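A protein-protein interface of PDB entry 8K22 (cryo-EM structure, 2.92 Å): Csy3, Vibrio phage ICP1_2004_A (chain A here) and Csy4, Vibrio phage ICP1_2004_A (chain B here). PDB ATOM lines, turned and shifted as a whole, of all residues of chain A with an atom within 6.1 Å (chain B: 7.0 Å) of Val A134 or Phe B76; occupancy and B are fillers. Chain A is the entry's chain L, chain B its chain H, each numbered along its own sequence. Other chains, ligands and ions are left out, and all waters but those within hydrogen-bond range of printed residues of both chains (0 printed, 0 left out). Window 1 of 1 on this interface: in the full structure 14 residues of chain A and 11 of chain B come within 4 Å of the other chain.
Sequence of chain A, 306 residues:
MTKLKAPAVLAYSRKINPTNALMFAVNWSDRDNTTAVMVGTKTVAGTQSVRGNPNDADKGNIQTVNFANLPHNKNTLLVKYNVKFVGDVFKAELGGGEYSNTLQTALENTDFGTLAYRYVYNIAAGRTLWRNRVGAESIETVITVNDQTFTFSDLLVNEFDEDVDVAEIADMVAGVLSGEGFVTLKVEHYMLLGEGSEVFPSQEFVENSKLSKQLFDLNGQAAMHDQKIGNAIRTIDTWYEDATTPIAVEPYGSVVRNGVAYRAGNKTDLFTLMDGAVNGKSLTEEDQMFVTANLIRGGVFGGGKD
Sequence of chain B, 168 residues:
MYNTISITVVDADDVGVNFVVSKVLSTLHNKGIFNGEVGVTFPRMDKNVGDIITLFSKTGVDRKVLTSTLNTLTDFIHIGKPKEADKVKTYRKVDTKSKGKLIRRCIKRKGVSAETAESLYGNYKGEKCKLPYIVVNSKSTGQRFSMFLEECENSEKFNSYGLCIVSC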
ATOM      1  N   LEU A 129     -10.605  11.145 -15.745  1.00  0.00           N
ATOM      2  CA  LEU A 129      -9.449  11.973 -15.409  1.00  0.00           C
ATOM      3  C   LEU A 129      -8.162  11.324 -15.907  1.00  0.00           C
ATOM      4  O   LEU A 129      -7.207  11.166 -15.150  1.00  0.00           O
ATOM      5  CB  LEU A 129      -9.343  12.212 -13.904  1.00  0.00           C
ATOM      6  CG  LEU A 129     -10.597  12.490 -13.087  1.00  0.00           C
ATOM      7  CD1 LEU A 129     -10.342  12.251 -11.615  1.00  0.00           C
ATOM      8  CD2 LEU A 129     -11.040  13.912 -13.346  1.00  0.00           C
ATOM      9  N   TRP A 130      -8.131  10.972 -17.198  1.00  0.00           N
ATOM     10  CA  TRP A 130      -7.189  10.052 -17.841  1.00  0.00           C
ATOM     11  C   TRP A 130      -5.718  10.253 -17.515  1.00  0.00           C
ATOM     12  O   TRP A 130      -5.085   9.382 -16.910  1.00  0.00           O
ATOM     13  CB  TRP A 130      -7.319  10.147 -19.359  1.00  0.00           C
ATOM     14  CG  TRP A 130      -8.578   9.593 -19.844  1.00  0.00           C
ATOM     15  CD1 TRP A 130      -8.785   8.362 -20.378  1.00  0.00           C
ATOM     16  CD2 TRP A 130      -9.829  10.262 -19.870  1.00  0.00           C
ATOM     17  NE1 TRP A 130     -10.103   8.212 -20.718  1.00  0.00           N
ATOM     18  CE2 TRP A 130     -10.762   9.372 -20.414  1.00  0.00           C
ATOM     19  CE3 TRP A 130     -10.257  11.535 -19.481  1.00  0.00           C
ATOM     20  CZ2 TRP A 130     -12.080   9.712 -20.584  1.00  0.00           C
ATOM     21  CZ3 TRP A 130     -11.568  11.863 -19.639  1.00  0.00           C
ATOM     22  CH2 TRP A 130     -12.470  10.956 -20.167  1.00  0.00           C
ATOM     23  N   ARG A 131      -5.172  11.399 -17.899  1.00  0.00           N
ATOM     24  CA  ARG A 131      -3.751  11.640 -17.743  1.00  0.00           C
ATOM     25  C   ARG A 131      -3.420  12.500 -16.536  1.00  0.00           C
ATOM     26  O   ARG A 131      -2.239  12.643 -16.206  1.00  0.00           O
ATOM     27  CB  ARG A 131      -3.183  12.290 -19.008  1.00  0.00           C
ATOM     28  CG  ARG A 131      -3.906  11.907 -20.284  1.00  0.00           C
ATOM     29  CD  ARG A 131      -3.302  12.599 -21.486  1.00  0.00           C
ATOM     30  NE  ARG A 131      -1.858  12.416 -21.542  1.00  0.00           N
ATOM     31  CZ  ARG A 131      -1.245  11.481 -22.253  1.00  0.00           C
ATOM     32  NH1 ARG A 131      -1.924  10.594 -22.961  1.00  0.00           N
ATOM     33  NH2 ARG A 131       0.083  11.434 -22.255  1.00  0.00           N
ATOM     34  N   ASN A 132      -4.420  13.072 -15.867  1.00  0.00           N
ATOM     35  CA  ASN A 132      -4.170  13.884 -14.687  1.00  0.00           C
ATOM     36  C   ASN A 132      -4.556  13.191 -13.388  1.00  0.00           C
ATOM     37  O   ASN A 132      -4.365  13.775 -12.318  1.00  0.00           O
ATOM     38  CB  ASN A 132      -4.884  15.236 -14.802  1.00  0.00           C
ATOM     39  CG  ASN A 132      -6.225  15.130 -15.474  1.00  0.00           C
ATOM     40  OD1 ASN A 132      -6.801  14.054 -15.552  1.00  0.00           O
ATOM     41  ND2 ASN A 132      -6.733  16.252 -15.967  1.00  0.00           N
ATOM     42  N   ARG A 133      -5.082  11.969 -13.438  1.00  0.00           N
ATOM     43  CA  ARG A 133      -5.064  11.145 -12.237  1.00  0.00           C
ATOM     44  C   ARG A 133      -3.772  10.358 -12.116  1.00  0.00           C
ATOM     45  O   ARG A 133      -3.525   9.750 -11.070  1.00  0.00           O
ATOM     46  CB  ARG A 133      -6.242  10.171 -12.205  1.00  0.00           C
ATOM     47  CG  ARG A 133      -6.054   8.946 -13.078  1.00  0.00           C
ATOM     48  CD  ARG A 133      -7.123   7.918 -12.799  1.00  0.00           C
ATOM     49  NE  ARG A 133      -7.599   7.284 -14.020  1.00  0.00           N
ATOM     50  CZ  ARG A 133      -7.266   6.062 -14.408  1.00  0.00           C
ATOM     51  NH1 ARG A 133      -6.446   5.311 -13.694  1.00  0.00           N
ATOM     52  NH2 ARG A 133      -7.771   5.581 -15.540  1.00  0.00           N
ATOM     53  N   VAL A 134      -2.955  10.363 -13.157  1.00  0.00           N
ATOM     54  CA  VAL A 134      -1.680   9.666 -13.146  1.00  0.00           C
ATOM     55  C   VAL A 134      -0.695  10.466 -12.310  1.00  0.00           C
ATOM     56  O   VAL A 134      -0.472  11.657 -12.558  1.00  0.00           O
ATOM     57  CB  VAL A 134      -1.168   9.481 -14.584  1.00  0.00           C
ATOM     58  CG1 VAL A 134       0.166   8.772 -14.591  1.00  0.00           C
ATOM     59  CG2 VAL A 134      -2.187   8.748 -15.426  1.00  0.00           C
ATOM     60  N   GLY A 135      -0.103   9.820 -11.313  1.00  0.00           N
ATOM     61  CA  GLY A 135       0.870  10.503 -10.489  1.00  0.00           C
ATOM     62  C   GLY A 135       0.301  11.410  -9.425  1.00  0.00           C
ATOM     63  O   GLY A 135       1.047  12.211  -8.854  1.00  0.00           O
ATOM     64  N   ALA A 136      -0.993  11.316  -9.135  1.00  0.00           N
ATOM     65  CA  ALA A 136      -1.605  12.116  -8.085  1.00  0.00           C
ATOM     66  C   ALA A 136      -1.569  11.342  -6.775  1.00  0.00           C
ATOM     67  O   ALA A 136      -1.994  10.185  -6.720  1.00  0.00           O
ATOM     68  CB  ALA A 136      -3.044  12.476  -8.449  1.00  0.00           C
ATOM     69  N   VAL A 157      -9.943   2.083 -10.242  1.00  0.00           N
ATOM     70  CA  VAL A 157     -10.855   2.342 -11.349  1.00  0.00           C
ATOM     71  C   VAL A 157     -11.039   1.123 -12.249  1.00  0.00           C
ATOM     72  O   VAL A 157     -12.074   1.009 -12.918  1.00  0.00           O
ATOM     73  CB  VAL A 157     -10.349   3.579 -12.119  1.00  0.00           C
ATOM     74  CG1 VAL A 157      -9.072   3.280 -12.894  1.00  0.00           C
ATOM     75  CG2 VAL A 157     -11.430   4.176 -13.008  1.00  0.00           C
ATOM     76  N   LEU A 193      -2.046  16.811  -7.324  1.00  0.00           N
ATOM     77  CA  LEU A 193      -0.918  16.411  -8.156  1.00  0.00           C
ATOM     78  C   LEU A 193       0.402  16.940  -7.617  1.00  0.00           C
ATOM     79  O   LEU A 193       1.439  16.280  -7.749  1.00  0.00           O
ATOM     80  CB  LEU A 193      -1.121  16.894  -9.586  1.00  0.00           C
ATOM     81  CG  LEU A 193      -2.278  16.284 -10.360  1.00  0.00           C
ATOM     82  CD1 LEU A 193      -3.271  17.349 -10.705  1.00  0.00           C
ATOM     83  CD2 LEU A 193      -1.730  15.653 -11.620  1.00  0.00           C
ATOM     84  N   THR B   8       6.510  -3.139 -14.351  1.00  0.00           N
ATOM     85  CA  THR B   8       5.830  -3.294 -15.626  1.00  0.00           C
ATOM     86  C   THR B   8       4.547  -2.483 -15.612  1.00  0.00           C
ATOM     87  O   THR B   8       3.726  -2.625 -14.700  1.00  0.00           O
ATOM     88  CB  THR B   8       5.514  -4.763 -15.905  1.00  0.00           C
ATOM     89  OG1 THR B   8       6.717  -5.537 -15.822  1.00  0.00           O
ATOM     90  CG2 THR B   8       4.909  -4.922 -17.287  1.00  0.00           C
ATOM     91  N   VAL B   9       4.384  -1.660 -16.649  1.00  0.00           N
ATOM     92  CA  VAL B   9       3.189  -0.851 -16.784  1.00  0.00           C
ATOM     93  C   VAL B   9       2.063  -1.668 -17.327  1.00  0.00           C
ATOM     94  O   VAL B   9       2.182  -2.263 -18.389  1.00  0.00           O
ATOM     95  CB  VAL B   9       3.447   0.316 -17.709  1.00  0.00           C
ATOM     96  CG1 VAL B   9       2.160   1.047 -18.002  1.00  0.00           C
ATOM     97  CG2 VAL B   9       4.457   1.251 -17.077  1.00  0.00           C
ATOM     98  N   VAL B  10       0.966  -1.724 -16.584  1.00  0.00           N
ATOM     99  CA  VAL B  10      -0.168  -2.517 -16.982  1.00  0.00           C
ATOM    100  C   VAL B  10      -1.307  -1.587 -17.229  1.00  0.00           C
ATOM    101  O   VAL B  10      -1.151  -0.405 -16.992  1.00  0.00           O
ATOM    102  CB  VAL B  10      -0.534  -3.494 -15.852  1.00  0.00           C
ATOM    103  CG1 VAL B  10       0.685  -3.754 -15.020  1.00  0.00           C
ATOM    104  CG2 VAL B  10      -1.575  -2.935 -14.895  1.00  0.00           C
ATOM    105  N   ASP B  11      -2.413  -2.077 -17.764  1.00  0.00           N
ATOM    106  CA  ASP B  11      -3.620  -1.279 -17.946  1.00  0.00           C
ATOM    107  C   ASP B  11      -3.443   0.182 -18.185  1.00  0.00           C
ATOM    108  O   ASP B  11      -4.002   1.007 -17.476  1.00  0.00           O
ATOM    109  CB  ASP B  11      -4.547  -1.474 -16.762  1.00  0.00           C
ATOM    110  CG  ASP B  11      -5.215  -2.829 -16.773  1.00  0.00           C
ATOM    111  OD1 ASP B  11      -5.566  -3.306 -17.872  1.00  0.00           O
ATOM    112  OD2 ASP B  11      -5.383  -3.418 -15.686  1.00  0.00           O
ATOM    113  N   ALA B  12      -2.681   0.510 -19.200  1.00  0.00           N
ATOM    114  CA  ALA B  12      -2.490   1.877 -19.534  1.00  0.00           C
ATOM    115  C   ALA B  12      -2.856   1.862 -20.964  1.00  0.00           C
ATOM    116  O   ALA B  12      -2.004   1.753 -21.832  1.00  0.00           O
ATOM    117  CB  ALA B  12      -1.048   2.230 -19.388  1.00  0.00           C
ATOM    118  N   ASP B  13      -4.138   1.947 -21.228  1.00  0.00           N
ATOM    119  CA  ASP B  13      -4.591   1.968 -22.586  1.00  0.00           C
ATOM    120  C   ASP B  13      -5.309   3.268 -22.666  1.00  0.00           C
ATOM    121  O   ASP B  13      -5.202   3.977 -23.653  1.00  0.00           O
ATOM    122  CB  ASP B  13      -5.549   0.819 -22.837  1.00  0.00           C
ATOM    123  CG  ASP B  13      -5.834   0.013 -21.581  1.00  0.00           C
ATOM    124  OD1 ASP B  13      -5.094  -0.955 -21.312  1.00  0.00           O
ATOM    125  OD2 ASP B  13      -6.797   0.352 -20.861  1.00  0.00           O
ATOM    126  N   ASP B  14      -6.011   3.613 -21.595  1.00  0.00           N
ATOM    127  CA  ASP B  14      -6.710   4.881 -21.556  1.00  0.00           C
ATOM    128  C   ASP B  14      -5.681   5.961 -21.661  1.00  0.00           C
ATOM    129  O   ASP B  14      -5.910   6.982 -22.296  1.00  0.00           O
ATOM    130  CB  ASP B  14      -7.580   5.003 -20.305  1.00  0.00           C
ATOM    131  CG  ASP B  14      -6.780   5.033 -19.022  1.00  0.00           C
ATOM    132  OD1 ASP B  14      -6.738   6.104 -18.380  1.00  0.00           O
ATOM    133  OD2 ASP B  14      -6.193   3.994 -18.655  1.00  0.00           O
ATOM    134  N   VAL B  15      -4.539   5.756 -21.036  1.00  0.00           N
ATOM    135  CA  VAL B  15      -3.462   6.681 -21.211  1.00  0.00           C
ATOM    136  C   VAL B  15      -2.447   5.841 -21.924  1.00  0.00           C
ATOM    137  O   VAL B  15      -2.401   4.668 -21.661  1.00  0.00           O
ATOM    138  CB  VAL B  15      -2.850   7.063 -19.877  1.00  0.00           C
ATOM    139  CG1 VAL B  15      -3.240   8.464 -19.531  1.00  0.00           C
ATOM    140  CG2 VAL B  15      -3.263   6.106 -18.773  1.00  0.00           C
ATOM    141  N   PHE B  19       3.392   7.208 -21.508  1.00  0.00           N
ATOM    142  CA  PHE B  19       3.146   8.264 -20.534  1.00  0.00           C
ATOM    143  C   PHE B  19       3.252   7.731 -19.112  1.00  0.00           C
ATOM    144  O   PHE B  19       3.809   8.396 -18.230  1.00  0.00           O
ATOM    145  CB  PHE B  19       1.776   8.891 -20.770  1.00  0.00           C
ATOM    146  CG  PHE B  19       1.362   9.846 -19.695  1.00  0.00           C
ATOM    147  CD1 PHE B  19       2.129  10.964 -19.417  1.00  0.00           C
ATOM    148  CD2 PHE B  19       0.212   9.625 -18.957  1.00  0.00           C
ATOM    149  CE1 PHE B  19       1.759  11.842 -18.425  1.00  0.00           C
ATOM    150  CE2 PHE B  19      -0.166  10.503 -17.965  1.00  0.00           C
ATOM    151  CZ  PHE B  19       0.608  11.615 -17.698  1.00  0.00           C
ATOM    152  N   VAL B  20       2.742   6.520 -18.878  1.00  0.00           N
ATOM    153  CA  VAL B  20       2.889   5.885 -17.573  1.00  0.00           C
ATOM    154  C   VAL B  20       4.345   5.531 -17.313  1.00  0.00           C
ATOM    155  O   VAL B  20       4.825   5.639 -16.182  1.00  0.00           O
ATOM    156  CB  VAL B  20       1.978   4.650 -17.473  1.00  0.00           C
ATOM    157  CG1 VAL B  20       1.923   4.149 -16.047  1.00  0.00           C
ATOM    158  CG2 VAL B  20       0.595   4.988 -17.956  1.00  0.00           C
ATOM    159  N   LYS B  23       6.031   8.769 -16.376  1.00  0.00           N
ATOM    160  CA  LYS B  23       5.651   9.160 -15.025  1.00  0.00           C
ATOM    161  C   LYS B  23       6.291   8.255 -13.976  1.00  0.00           C
ATOM    162  O   LYS B  23       6.608   8.721 -12.878  1.00  0.00           O
ATOM    163  CB  LYS B  23       4.127   9.161 -14.891  1.00  0.00           C
ATOM    164  CG  LYS B  23       3.605   9.720 -13.576  1.00  0.00           C
ATOM    165  CD  LYS B  23       3.981  11.183 -13.397  1.00  0.00           C
ATOM    166  CE  LYS B  23       3.370  12.053 -14.482  1.00  0.00           C
ATOM    167  NZ  LYS B  23       1.901  11.850 -14.586  1.00  0.00           N
ATOM    168  N   VAL B  24       6.510   6.978 -14.307  1.00  0.00           N
ATOM    169  CA  VAL B  24       7.267   6.082 -13.435  1.00  0.00           C
ATOM    170  C   VAL B  24       8.705   6.563 -13.294  1.00  0.00           C
ATOM    171  O   VAL B  24       9.252   6.595 -12.186  1.00  0.00           O
ATOM    172  CB  VAL B  24       7.180   4.633 -13.957  1.00  0.00           C
ATOM    173  CG1 VAL B  24       8.294   3.767 -13.404  1.00  0.00           C
ATOM    174  CG2 VAL B  24       5.856   4.025 -13.550  1.00  0.00           C
ATOM    175  N   THR B  72       1.609   6.329  -6.244  1.00  0.00           N
ATOM    176  CA  THR B  72       0.765   7.099  -7.142  1.00  0.00           C
ATOM    177  C   THR B  72       0.430   6.355  -8.428  1.00  0.00           C
ATOM    178  O   THR B  72      -0.566   6.691  -9.075  1.00  0.00           O
ATOM    179  CB  THR B  72       1.454   8.419  -7.475  1.00  0.00           C
ATOM    180  OG1 THR B  72       2.777   8.156  -7.951  1.00  0.00           O
ATOM    181  CG2 THR B  72       1.575   9.265  -6.238  1.00  0.00           C
ATOM    182  N   LEU B  73       1.228   5.360  -8.813  1.00  0.00           N
ATOM    183  CA  LEU B  73       1.010   4.627 -10.055  1.00  0.00           C
ATOM    184  C   LEU B  73       0.430   3.237  -9.835  1.00  0.00           C
ATOM    185  O   LEU B  73       0.327   2.471 -10.796  1.00  0.00           O
ATOM    186  CB  LEU B  73       2.307   4.496 -10.859  1.00  0.00           C
ATOM    187  CG  LEU B  73       3.026   5.692 -11.493  1.00  0.00           C
ATOM    188  CD1 LEU B  73       2.043   6.578 -12.228  1.00  0.00           C
ATOM    189  CD2 LEU B  73       3.883   6.480 -10.526  1.00  0.00           C
ATOM    190  N   THR B  74       0.021   2.907  -8.606  1.00  0.00           N
ATOM    191  CA  THR B  74      -0.367   1.553  -8.217  1.00  0.00           C
ATOM    192  C   THR B  74      -1.613   1.053  -8.948  1.00  0.00           C
ATOM    193  O   THR B  74      -1.806  -0.165  -9.052  1.00  0.00           O
ATOM    194  CB  THR B  74      -0.578   1.525  -6.697  1.00  0.00           C
ATOM    195  OG1 THR B  74       0.481   2.252  -6.070  1.00  0.00           O
ATOM    196  CG2 THR B  74      -0.535   0.105  -6.138  1.00  0.00           C
ATOM    197  N   ASP B  75      -2.429   1.960  -9.494  1.00  0.00           N
ATOM    198  CA  ASP B  75      -3.621   1.562 -10.237  1.00  0.00           C
ATOM    199  C   ASP B  75      -3.263   0.815 -11.517  1.00  0.00           C
ATOM    200  O   ASP B  75      -3.998  -0.081 -11.947  1.00  0.00           O
ATOM    201  CB  ASP B  75      -4.464   2.796 -10.558  1.00  0.00           C
ATOM    202  CG  ASP B  75      -5.952   2.505 -10.561  1.00  0.00           C
ATOM    203  OD1 ASP B  75      -6.357   1.453 -11.096  1.00  0.00           O
ATOM    204  OD2 ASP B  75      -6.720   3.336 -10.031  1.00  0.00           O
ATOM    205  N   PHE B  76      -2.140   1.163 -12.137  1.00  0.00           N
ATOM    206  CA  PHE B  76      -1.724   0.557 -13.399  1.00  0.00           C
ATOM    207  C   PHE B  76      -0.231   0.243 -13.385  1.00  0.00           C
ATOM    208  O   PHE B  76       0.508   0.577 -14.310  1.00  0.00           O
ATOM    209  CB  PHE B  76      -2.086   1.442 -14.593  1.00  0.00           C
ATOM    210  CG  PHE B  76      -2.058   2.911 -14.294  1.00  0.00           C
ATOM    211  CD1 PHE B  76      -0.888   3.537 -13.903  1.00  0.00           C
ATOM    212  CD2 PHE B  76      -3.212   3.663 -14.404  1.00  0.00           C
ATOM    213  CE1 PHE B  76      -0.871   4.880 -13.625  1.00  0.00           C
ATOM    214  CE2 PHE B  76      -3.200   5.008 -14.129  1.00  0.00           C
ATOM    215  CZ  PHE B  76      -2.029   5.614 -13.735  1.00  0.00           C
ATOM    216  N   ILE B  77       0.234  -0.399 -12.316  1.00  0.00           N
ATOM    217  CA  ILE B  77       1.613  -0.854 -12.236  1.00  0.00           C
ATOM    218  C   ILE B  77       1.631  -2.287 -11.719  1.00  0.00           C
ATOM    219  O   ILE B  77       0.669  -2.771 -11.117  1.00  0.00           O
ATOM    220  CB  ILE B  77       2.481   0.079 -11.356  1.00  0.00           C
ATOM    221  CG1 ILE B  77       3.883   0.198 -11.936  1.00  0.00           C
ATOM    222  CG2 ILE B  77       2.512  -0.359  -9.892  1.00  0.00           C
ATOM    223  CD1 ILE B  77       3.906   0.828 -13.299  1.00  0.00           C
ATOM    224  N   HIS B  78       2.730  -2.979 -12.003  1.00  0.00           N
ATOM    225  CA  HIS B  78       2.967  -4.311 -11.477  1.00  0.00           C
ATOM    226  C   HIS B  78       4.443  -4.442 -11.147  1.00  0.00           C
ATOM    227  O   HIS B  78       5.297  -4.042 -11.938  1.00  0.00           O
ATOM    228  CB  HIS B  78       2.537  -5.385 -12.478  1.00  0.00           C
ATOM    229  CG  HIS B  78       3.146  -6.724 -12.226  1.00  0.00           C
ATOM    230  ND1 HIS B  78       4.289  -7.153 -12.863  1.00  0.00           N
ATOM    231  CD2 HIS B  78       2.784  -7.723 -11.389  1.00  0.00           C
ATOM    232  CE1 HIS B  78       4.597  -8.364 -12.439  1.00  0.00           C
ATOM    233  NE2 HIS B  78       3.697  -8.735 -11.547  1.00  0.00           N
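The side-chain carboxylate (OD1) of Asp B14 is in salt-bridge range of the guanidinium group (NH2) of Arg A133, 3.1 Å away. The backbone carbonyl oxygen (O) of Val A134 lies within hydrogen-bond range of the side-chain amino group (NZ) of Lys B23 (3.1 Å). N of Val A157 is in hydrogen-bond range of OD2 of Asp B75 (3.5 Å).
The backbone carbonyl oxygen (O) of Phe B76 lies within hydrogen-bond range of the backbone NH (N) of Val B10 (3.3 Å).
Trp A130 touches Asp B14. Val B15 touches Trp A130 (CG1 to O, 3.3 Å). Val B15 touches Arg A131. Arg A133 touches Phe B76 (NH1 to CE2, 3.3 Å). CE2 of Phe B19 touches CB of Val A134 (3.7 Å). Val A134 touches Leu B73 (CG1 to CD1, 3.7 Å). Phe B76 touches Val A134 (CZ to CG2, 3.6 Å). CA of Gly A135 touches CB of Thr B72, 3.7 Å away. Gly A135 touches Leu B73. O of Ala A136 touches CG2 of Thr B72, 3.7 Å away.
Leu A129 touches none of the printed residues of chain B. Of the printed residues of chain B, Arg A133 touches Asp B14 and Phe B76. Of chain B, only Phe B19 (3.7 Å), Lys B23 (3.1 Å), Leu B73 (3.7 Å) and Phe B76 (3.6 Å) come within 4 Å of Val A134. Ala B12 touches none of the printed residues of chain A. Of the printed residues of chain A, Asp B14 touches Trp A130 (3.6 Å) and Arg A133 (3.1 Å). Of the printed residues of chain A, Phe B19 touches Arg A131 (3.3 Å) and Val A134 (3.7 Å). Of the printed residues of chain A, Lys B23 touches Val A134 (3.1 Å). Printed residues of chain A within 4 Å of Thr B72: Gly A135 (3.7 Å) and Ala A136 (3.7 Å). Phe B76 touches two residues of chain A. The nearest residue of chain B that does not touch Val A134 is Val B15 (4.2 Å). The nearest printed residue of chain B that does not touch Val A157 is Phe B76 (6.1 Å).
Printed residues of chain A that touch a printed residue of chain B: Trp A130, Arg A131, Arg A133, Val A134, Gly A135, Ala A136 and Val A157. Hydrophobic or aromatic side chains of chain A within 4 Å of the printed part of chain B: Trp A130, Val A134 and Val A157. Of the 19 printed residues of chain B, 8 touch a printed residue of chain A. Among the printed residues, Asp or Glu carboxylates within 4 Å of a Lys or Arg side-chain nitrogen of the other chain: Arg A133 with Asp B14 (3.1 Å).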
